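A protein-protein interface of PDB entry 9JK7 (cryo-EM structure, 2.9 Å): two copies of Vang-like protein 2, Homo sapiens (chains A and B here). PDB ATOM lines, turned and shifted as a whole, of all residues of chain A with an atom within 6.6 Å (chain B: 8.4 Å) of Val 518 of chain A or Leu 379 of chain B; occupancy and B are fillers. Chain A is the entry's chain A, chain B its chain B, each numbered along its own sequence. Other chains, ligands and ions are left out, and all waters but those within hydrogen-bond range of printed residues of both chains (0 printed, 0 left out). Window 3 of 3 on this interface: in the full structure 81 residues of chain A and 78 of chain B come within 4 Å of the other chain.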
ATOM      1  N   SER A 514     -17.607  20.060  19.206  1.00  0.00           N
ATOM      2  CA  SER A 514     -16.974  21.244  18.642  1.00  0.00           C
ATOM      3  C   SER A 514     -17.821  21.939  17.585  1.00  0.00           C
ATOM      4  O   SER A 514     -17.360  22.921  16.994  1.00  0.00           O
ATOM      5  CB  SER A 514     -15.618  20.874  18.038  1.00  0.00           C
ATOM      6  OG  SER A 514     -15.782  20.011  16.928  1.00  0.00           O
ATOM      7  N   LYS A 516     -20.279  24.463  16.589  1.00  0.00           N
ATOM      8  CA  LYS A 516     -20.865  25.670  17.150  1.00  0.00           C
ATOM      9  C   LYS A 516     -21.209  26.632  16.023  1.00  0.00           C
ATOM     10  O   LYS A 516     -20.362  26.952  15.189  1.00  0.00           O
ATOM     11  CB  LYS A 516     -19.910  26.341  18.141  1.00  0.00           C
ATOM     12  CG  LYS A 516     -19.513  25.464  19.318  1.00  0.00           C
ATOM     13  CD  LYS A 516     -20.694  25.173  20.228  1.00  0.00           C
ATOM     14  CE  LYS A 516     -20.262  24.365  21.440  1.00  0.00           C
ATOM     15  NZ  LYS A 516     -21.403  24.041  22.339  1.00  0.00           N
ATOM     16  N   PHE A 517     -22.459  27.096  16.004  1.00  0.00           N
ATOM     17  CA  PHE A 517     -22.980  27.841  14.863  1.00  0.00           C
ATOM     18  C   PHE A 517     -23.366  29.249  15.300  1.00  0.00           C
ATOM     19  O   PHE A 517     -23.505  29.534  16.490  1.00  0.00           O
ATOM     20  CB  PHE A 517     -24.189  27.134  14.234  1.00  0.00           C
ATOM     21  CG  PHE A 517     -23.875  25.776  13.664  1.00  0.00           C
ATOM     22  CD1 PHE A 517     -22.573  25.343  13.528  1.00  0.00           C
ATOM     23  CD2 PHE A 517     -24.884  24.944  13.241  1.00  0.00           C
ATOM     24  CE1 PHE A 517     -22.290  24.101  13.016  1.00  0.00           C
ATOM     25  CE2 PHE A 517     -24.600  23.707  12.719  1.00  0.00           C
ATOM     26  CZ  PHE A 517     -23.303  23.288  12.606  1.00  0.00           C
ATOM     27  N   VAL A 518     -23.530  30.139  14.315  1.00  0.00           N
ATOM     28  CA  VAL A 518     -23.897  31.529  14.565  1.00  0.00           C
ATOM     29  C   VAL A 518     -24.967  31.968  13.573  1.00  0.00           C
ATOM     30  O   VAL A 518     -25.283  31.258  12.613  1.00  0.00           O
ATOM     31  CB  VAL A 518     -22.681  32.481  14.501  1.00  0.00           C
ATOM     32  CG1 VAL A 518     -21.697  32.169  15.614  1.00  0.00           C
ATOM     33  CG2 VAL A 518     -22.003  32.390  13.149  1.00  0.00           C
ATOM     34  N   MET A 519     -25.526  33.158  13.819  1.00  0.00           N
ATOM     35  CA  MET A 519     -26.748  33.583  13.138  1.00  0.00           C
ATOM     36  C   MET A 519     -26.553  33.759  11.636  1.00  0.00           C
ATOM     37  O   MET A 519     -27.114  33.007  10.834  1.00  0.00           O
ATOM     38  CB  MET A 519     -27.252  34.893  13.743  1.00  0.00           C
ATOM     39  CG  MET A 519     -27.751  34.806  15.171  1.00  0.00           C
ATOM     40  SD  MET A 519     -29.193  33.744  15.351  1.00  0.00           S
ATOM     41  CE  MET A 519     -28.443  32.320  16.121  1.00  0.00           C
ATOM     42  N   ARG A 520     -25.758  34.745  11.234  1.00  0.00           N
ATOM     43  CA  ARG A 520     -25.852  35.287   9.883  1.00  0.00           C
ATOM     44  C   ARG A 520     -25.117  34.426   8.867  1.00  0.00           C
ATOM     45  O   ARG A 520     -23.989  33.989   9.107  1.00  0.00           O
ATOM     46  CB  ARG A 520     -25.309  36.717   9.836  1.00  0.00           C
ATOM     47  CG  ARG A 520     -26.306  37.782  10.288  1.00  0.00           C
ATOM     48  CD  ARG A 520     -26.323  37.932  11.799  1.00  0.00           C
ATOM     49  NE  ARG A 520     -25.047  38.430  12.302  1.00  0.00           N
ATOM     50  CZ  ARG A 520     -24.691  38.422  13.582  1.00  0.00           C
ATOM     51  NH1 ARG A 520     -25.519  37.942  14.500  1.00  0.00           N
ATOM     52  NH2 ARG A 520     -23.507  38.895  13.945  1.00  0.00           N
ATOM     53  N   LEU A 521     -25.766  34.215   7.721  1.00  0.00           N
ATOM     54  CA  LEU A 521     -25.220  33.498   6.562  1.00  0.00           C
ATOM     55  C   LEU A 521     -24.388  32.270   6.921  1.00  0.00           C
ATOM     56  O   LEU A 521     -24.050  31.465   6.053  1.00  0.00           O
ATOM     57  CB  LEU A 521     -24.394  34.455   5.688  1.00  0.00           C
ATOM     58  CG  LEU A 521     -23.143  35.167   6.221  1.00  0.00           C
ATOM     59  CD1 LEU A 521     -21.892  34.317   6.052  1.00  0.00           C
ATOM     60  CD2 LEU A 521     -22.969  36.521   5.547  1.00  0.00           C
ATOM     61  N   PHE B 373     -31.117  26.961   5.553  1.00  0.00           N
ATOM     62  CA  PHE B 373     -29.707  26.695   5.804  1.00  0.00           C
ATOM     63  C   PHE B 373     -28.859  27.951   5.648  1.00  0.00           C
ATOM     64  O   PHE B 373     -27.805  28.060   6.280  1.00  0.00           O
ATOM     65  CB  PHE B 373     -29.180  25.577   4.902  1.00  0.00           C
ATOM     66  CG  PHE B 373     -29.660  24.205   5.290  1.00  0.00           C
ATOM     67  CD1 PHE B 373     -30.463  24.024   6.396  1.00  0.00           C
ATOM     68  CD2 PHE B 373     -29.238  23.090   4.599  1.00  0.00           C
ATOM     69  CE1 PHE B 373     -30.887  22.764   6.761  1.00  0.00           C
ATOM     70  CE2 PHE B 373     -29.654  21.828   4.968  1.00  0.00           C
ATOM     71  CZ  PHE B 373     -30.478  21.667   6.049  1.00  0.00           C
ATOM     72  N   THR B 374     -29.294  28.909   4.824  1.00  0.00           N
ATOM     73  CA  THR B 374     -28.595  30.188   4.807  1.00  0.00           C
ATOM     74  C   THR B 374     -28.842  30.997   6.071  1.00  0.00           C
ATOM     75  O   THR B 374     -28.111  31.959   6.325  1.00  0.00           O
ATOM     76  CB  THR B 374     -28.998  31.020   3.588  1.00  0.00           C
ATOM     77  OG1 THR B 374     -30.412  31.244   3.603  1.00  0.00           O
ATOM     78  CG2 THR B 374     -28.595  30.323   2.299  1.00  0.00           C
ATOM     79  N   HIS B 375     -29.854  30.640   6.866  1.00  0.00           N
ATOM     80  CA  HIS B 375     -30.108  31.365   8.106  1.00  0.00           C
ATOM     81  C   HIS B 375     -29.149  31.004   9.237  1.00  0.00           C
ATOM     82  O   HIS B 375     -29.370  31.461  10.362  1.00  0.00           O
ATOM     83  CB  HIS B 375     -31.541  31.129   8.584  1.00  0.00           C
ATOM     84  CG  HIS B 375     -32.578  31.825   7.761  1.00  0.00           C
ATOM     85  ND1 HIS B 375     -33.925  31.583   7.903  1.00  0.00           N
ATOM     86  CD2 HIS B 375     -32.464  32.766   6.793  1.00  0.00           C
ATOM     87  CE1 HIS B 375     -34.599  32.338   7.053  1.00  0.00           C
ATOM     88  NE2 HIS B 375     -33.735  33.066   6.369  1.00  0.00           N
ATOM     89  N   ILE B 376     -28.118  30.193   8.986  1.00  0.00           N
ATOM     90  CA  ILE B 376     -27.106  29.876   9.986  1.00  0.00           C
ATOM     91  C   ILE B 376     -25.741  29.755   9.321  1.00  0.00           C
ATOM     92  O   ILE B 376     -25.622  29.486   8.125  1.00  0.00           O
ATOM     93  CB  ILE B 376     -27.410  28.582  10.778  1.00  0.00           C
ATOM     94  CG1 ILE B 376     -27.669  27.414   9.823  1.00  0.00           C
ATOM     95  CG2 ILE B 376     -28.512  28.807  11.803  1.00  0.00           C
ATOM     96  CD1 ILE B 376     -27.700  26.070  10.502  1.00  0.00           C
ATOM     97  N   LYS B 377     -24.703  29.941  10.134  1.00  0.00           N
ATOM     98  CA  LYS B 377     -23.320  29.906   9.684  1.00  0.00           C
ATOM     99  C   LYS B 377     -22.550  28.890  10.514  1.00  0.00           C
ATOM    100  O   LYS B 377     -22.890  28.624  11.669  1.00  0.00           O
ATOM    101  CB  LYS B 377     -22.667  31.290   9.799  1.00  0.00           C
ATOM    102  CG  LYS B 377     -21.276  31.408   9.203  1.00  0.00           C
ATOM    103  CD  LYS B 377     -20.756  32.832   9.326  1.00  0.00           C
ATOM    104  CE  LYS B 377     -19.362  32.972   8.736  1.00  0.00           C
ATOM    105  NZ  LYS B 377     -18.845  34.361   8.864  1.00  0.00           N
ATOM    106  N   ARG B 378     -21.503  28.324   9.911  1.00  0.00           N
ATOM    107  CA  ARG B 378     -20.763  27.250  10.561  1.00  0.00           C
ATOM    108  C   ARG B 378     -19.892  27.741  11.712  1.00  0.00           C
ATOM    109  O   ARG B 378     -19.633  26.969  12.640  1.00  0.00           O
ATOM    110  CB  ARG B 378     -19.907  26.510   9.529  1.00  0.00           C
ATOM    111  CG  ARG B 378     -19.075  25.393  10.120  1.00  0.00           C
ATOM    112  CD  ARG B 378     -19.980  24.351  10.732  1.00  0.00           C
ATOM    113  NE  ARG B 378     -19.238  23.329  11.458  1.00  0.00           N
ATOM    114  CZ  ARG B 378     -18.825  22.192  10.921  1.00  0.00           C
ATOM    115  NH1 ARG B 378     -19.089  21.932   9.652  1.00  0.00           N
ATOM    116  NH2 ARG B 378     -18.153  21.314  11.650  1.00  0.00           N
ATOM    117  N   LEU B 379     -19.458  28.999  11.688  1.00  0.00           N
ATOM    118  CA  LEU B 379     -18.520  29.529  12.680  1.00  0.00           C
ATOM    119  C   LEU B 379     -17.259  28.674  12.769  1.00  0.00           C
ATOM    120  O   LEU B 379     -17.169  27.756  13.584  1.00  0.00           O
ATOM    121  CB  LEU B 379     -19.172  29.634  14.061  1.00  0.00           C
ATOM    122  CG  LEU B 379     -18.286  30.207  15.172  1.00  0.00           C
ATOM    123  CD1 LEU B 379     -17.911  31.650  14.881  1.00  0.00           C
ATOM    124  CD2 LEU B 379     -18.953  30.078  16.533  1.00  0.00           C
ATOM    125  N   VAL B 390     -23.118  32.041  20.240  1.00  0.00           N
ATOM    126  CA  VAL B 390     -22.806  30.639  19.999  1.00  0.00           C
ATOM    127  C   VAL B 390     -24.112  29.854  20.018  1.00  0.00           C
ATOM    128  O   VAL B 390     -25.101  30.313  20.586  1.00  0.00           O
ATOM    129  CB  VAL B 390     -21.799  30.105  21.038  1.00  0.00           C
ATOM    130  CG1 VAL B 390     -22.446  29.999  22.412  1.00  0.00           C
ATOM    131  CG2 VAL B 390     -21.205  28.777  20.595  1.00  0.00           C
ATOM    132  N   MET B 391     -24.119  28.677  19.394  1.00  0.00           N
ATOM    133  CA  MET B 391     -25.345  27.906  19.250  1.00  0.00           C
ATOM    134  C   MET B 391     -25.003  26.481  18.844  1.00  0.00           C
ATOM    135  O   MET B 391     -24.195  26.271  17.937  1.00  0.00           O
ATOM    136  CB  MET B 391     -26.269  28.570  18.222  1.00  0.00           C
ATOM    137  CG  MET B 391     -27.556  27.843  17.946  1.00  0.00           C
ATOM    138  SD  MET B 391     -28.640  28.836  16.911  1.00  0.00           S
ATOM    139  CE  MET B 391     -27.707  28.888  15.388  1.00  0.00           C
ATOM    140  N   ASP B 392     -25.614  25.511  19.523  1.00  0.00           N
ATOM    141  CA  ASP B 392     -25.371  24.103  19.256  1.00  0.00           C
ATOM    142  C   ASP B 392     -26.058  23.681  17.957  1.00  0.00           C
ATOM    143  O   ASP B 392     -26.928  24.392  17.448  1.00  0.00           O
ATOM    144  CB  ASP B 392     -25.880  23.261  20.423  1.00  0.00           C
ATOM    145  CG  ASP B 392     -25.069  23.466  21.686  1.00  0.00           C
ATOM    146  OD1 ASP B 392     -23.867  23.779  21.574  1.00  0.00           O
ATOM    147  OD2 ASP B 392     -25.634  23.317  22.788  1.00  0.00           O
ATOM    148  N   ALA B 396     -29.487  25.130  16.438  1.00  0.00           N
ATOM    149  CA  ALA B 396     -29.473  25.683  15.089  1.00  0.00           C
ATOM    150  C   ALA B 396     -30.506  25.007  14.203  1.00  0.00           C
ATOM    151  O   ALA B 396     -31.159  25.666  13.386  1.00  0.00           O
ATOM    152  CB  ALA B 396     -28.084  25.542  14.480  1.00  0.00           C
ATOM    153  N   ALA B 399     -33.701  26.459  15.122  1.00  0.00           N
ATOM    154  CA  ALA B 399     -33.835  27.848  14.702  1.00  0.00           C
ATOM    155  C   ALA B 399     -34.080  27.958  13.202  1.00  0.00           C
ATOM    156  O   ALA B 399     -34.741  28.895  12.745  1.00  0.00           O
ATOM    157  CB  ALA B 399     -32.590  28.636  15.100  1.00  0.00           C
ATOM    158  N   ILE B 400     -33.549  27.017  12.418  1.00  0.00           N
ATOM    159  CA  ILE B 400     -33.780  27.031  10.975  1.00  0.00           C
ATOM    160  C   ILE B 400     -34.990  26.211  10.561  1.00  0.00           C
ATOM    161  O   ILE B 400     -35.407  26.291   9.397  1.00  0.00           O
ATOM    162  CB  ILE B 400     -32.555  26.516  10.197  1.00  0.00           C
ATOM    163  CG1 ILE B 400     -32.274  25.059  10.546  1.00  0.00           C
ATOM    164  CG2 ILE B 400     -31.351  27.363  10.494  1.00  0.00           C
ATOM    165  CD1 ILE B 400     -31.180  24.449   9.729  1.00  0.00           C
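Among the printed residues, pairs that only touch across the chains: Arg 520 of chain A with Lys 377 of chain B (3.1 Å), Lys 516 of chain A with Leu 379 of chain B (3.1 Å), Phe 517 of chain A with Lys 377 of chain B (3.2 Å), Met 519 of chain A with Ile 376 of chain B (3.2 Å), Phe 517 of chain A with Arg 378 of chain B (3.3 Å), Leu 521 of chain A with Thr 374 of chain B (3.3 Å), Lys 516 of chain A with Met 391 of chain B (3.5 Å), Phe 517 of chain A with Ala 396 of chain B (3.5 Å), Val 518 of chain A with Ile 376 of chain B (3.5 Å), Leu 521 of chain A with Lys 377 of chain B (3.5 Å), Val 518 of chain A with Leu 379 of chain B (3.6 Å), Met 519 of chain A with Met 391 of chain B (3.6 Å), Phe 517 of chain A with Val 390 of chain B (3.6 Å), Lys 516 of chain A with Val 390 of chain B (3.7 Å) and Met 519 of chain A with Lys 377 of chain B (3.96 Å).
Val 518 of chain A touches three residues of chain B.
Of the printed residues of chain A, Thr 374 of chain B touches Leu 521.
Printed residues of chain A within 4 Å of His 375 of chain B: Met 519 (2.8 Å).
Of chain A, only Lys 516 and Val 518 come within 4 Å of Leu 379 of chain B.
The nearest residue of chain B that does not touch Val 518 of chain A is Met 391 of chain B (4.4 Å).
Of the 7 printed residues of chain A, 6 touch a printed residue of chain B.
Of the 13 printed residues of chain B, 10 touch a printed residue of chain A.
Hydrophobic or aromatic side chains of chain B that line the printed part of chain A: Ile 376, Leu 379, Val 390, Met 391 and Ala 396.
Among the printed residues, 21 pairs touch across the chains.
Among the printed residues, Asp or Glu carboxylates within 4 Å of a Lys or Arg side-chain nitrogen of the other chain: Lys 516 of chain A with Asp 392 of chain B (2.6 Å).
N of Phe 517 of chain A sits at hydrogen-bond distance from O of Met 391 of chain B, 2.7 Å away.
O of Lys 516 of chain A lies close to O of Arg 378 of chain B, at 2.7 Å.
NZ of Lys 516 of chain A is in salt-bridge range of OD1 of Asp 392 of chain B (2.6 Å).
O of Ile 376 of chain B sits close to O of Leu 521 of chain A (3.3 Å).
The backbone NH (N) of Lys 377 of chain B is in hydrogen-bond range of the backbone carbonyl oxygen (O) of Val 518 of chain A, at 2.9 Å.
The backbone carbonyl oxygen (O) of Met 519 of chain A lies close to the backbone carbonyl oxygen (O) of His 375 of chain B, 2.8 Å away.
No position is printed for both chains.
Of the 21 pairs that touch across the chains among the printed residues, none has its exchanged pair printed and touching as well.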
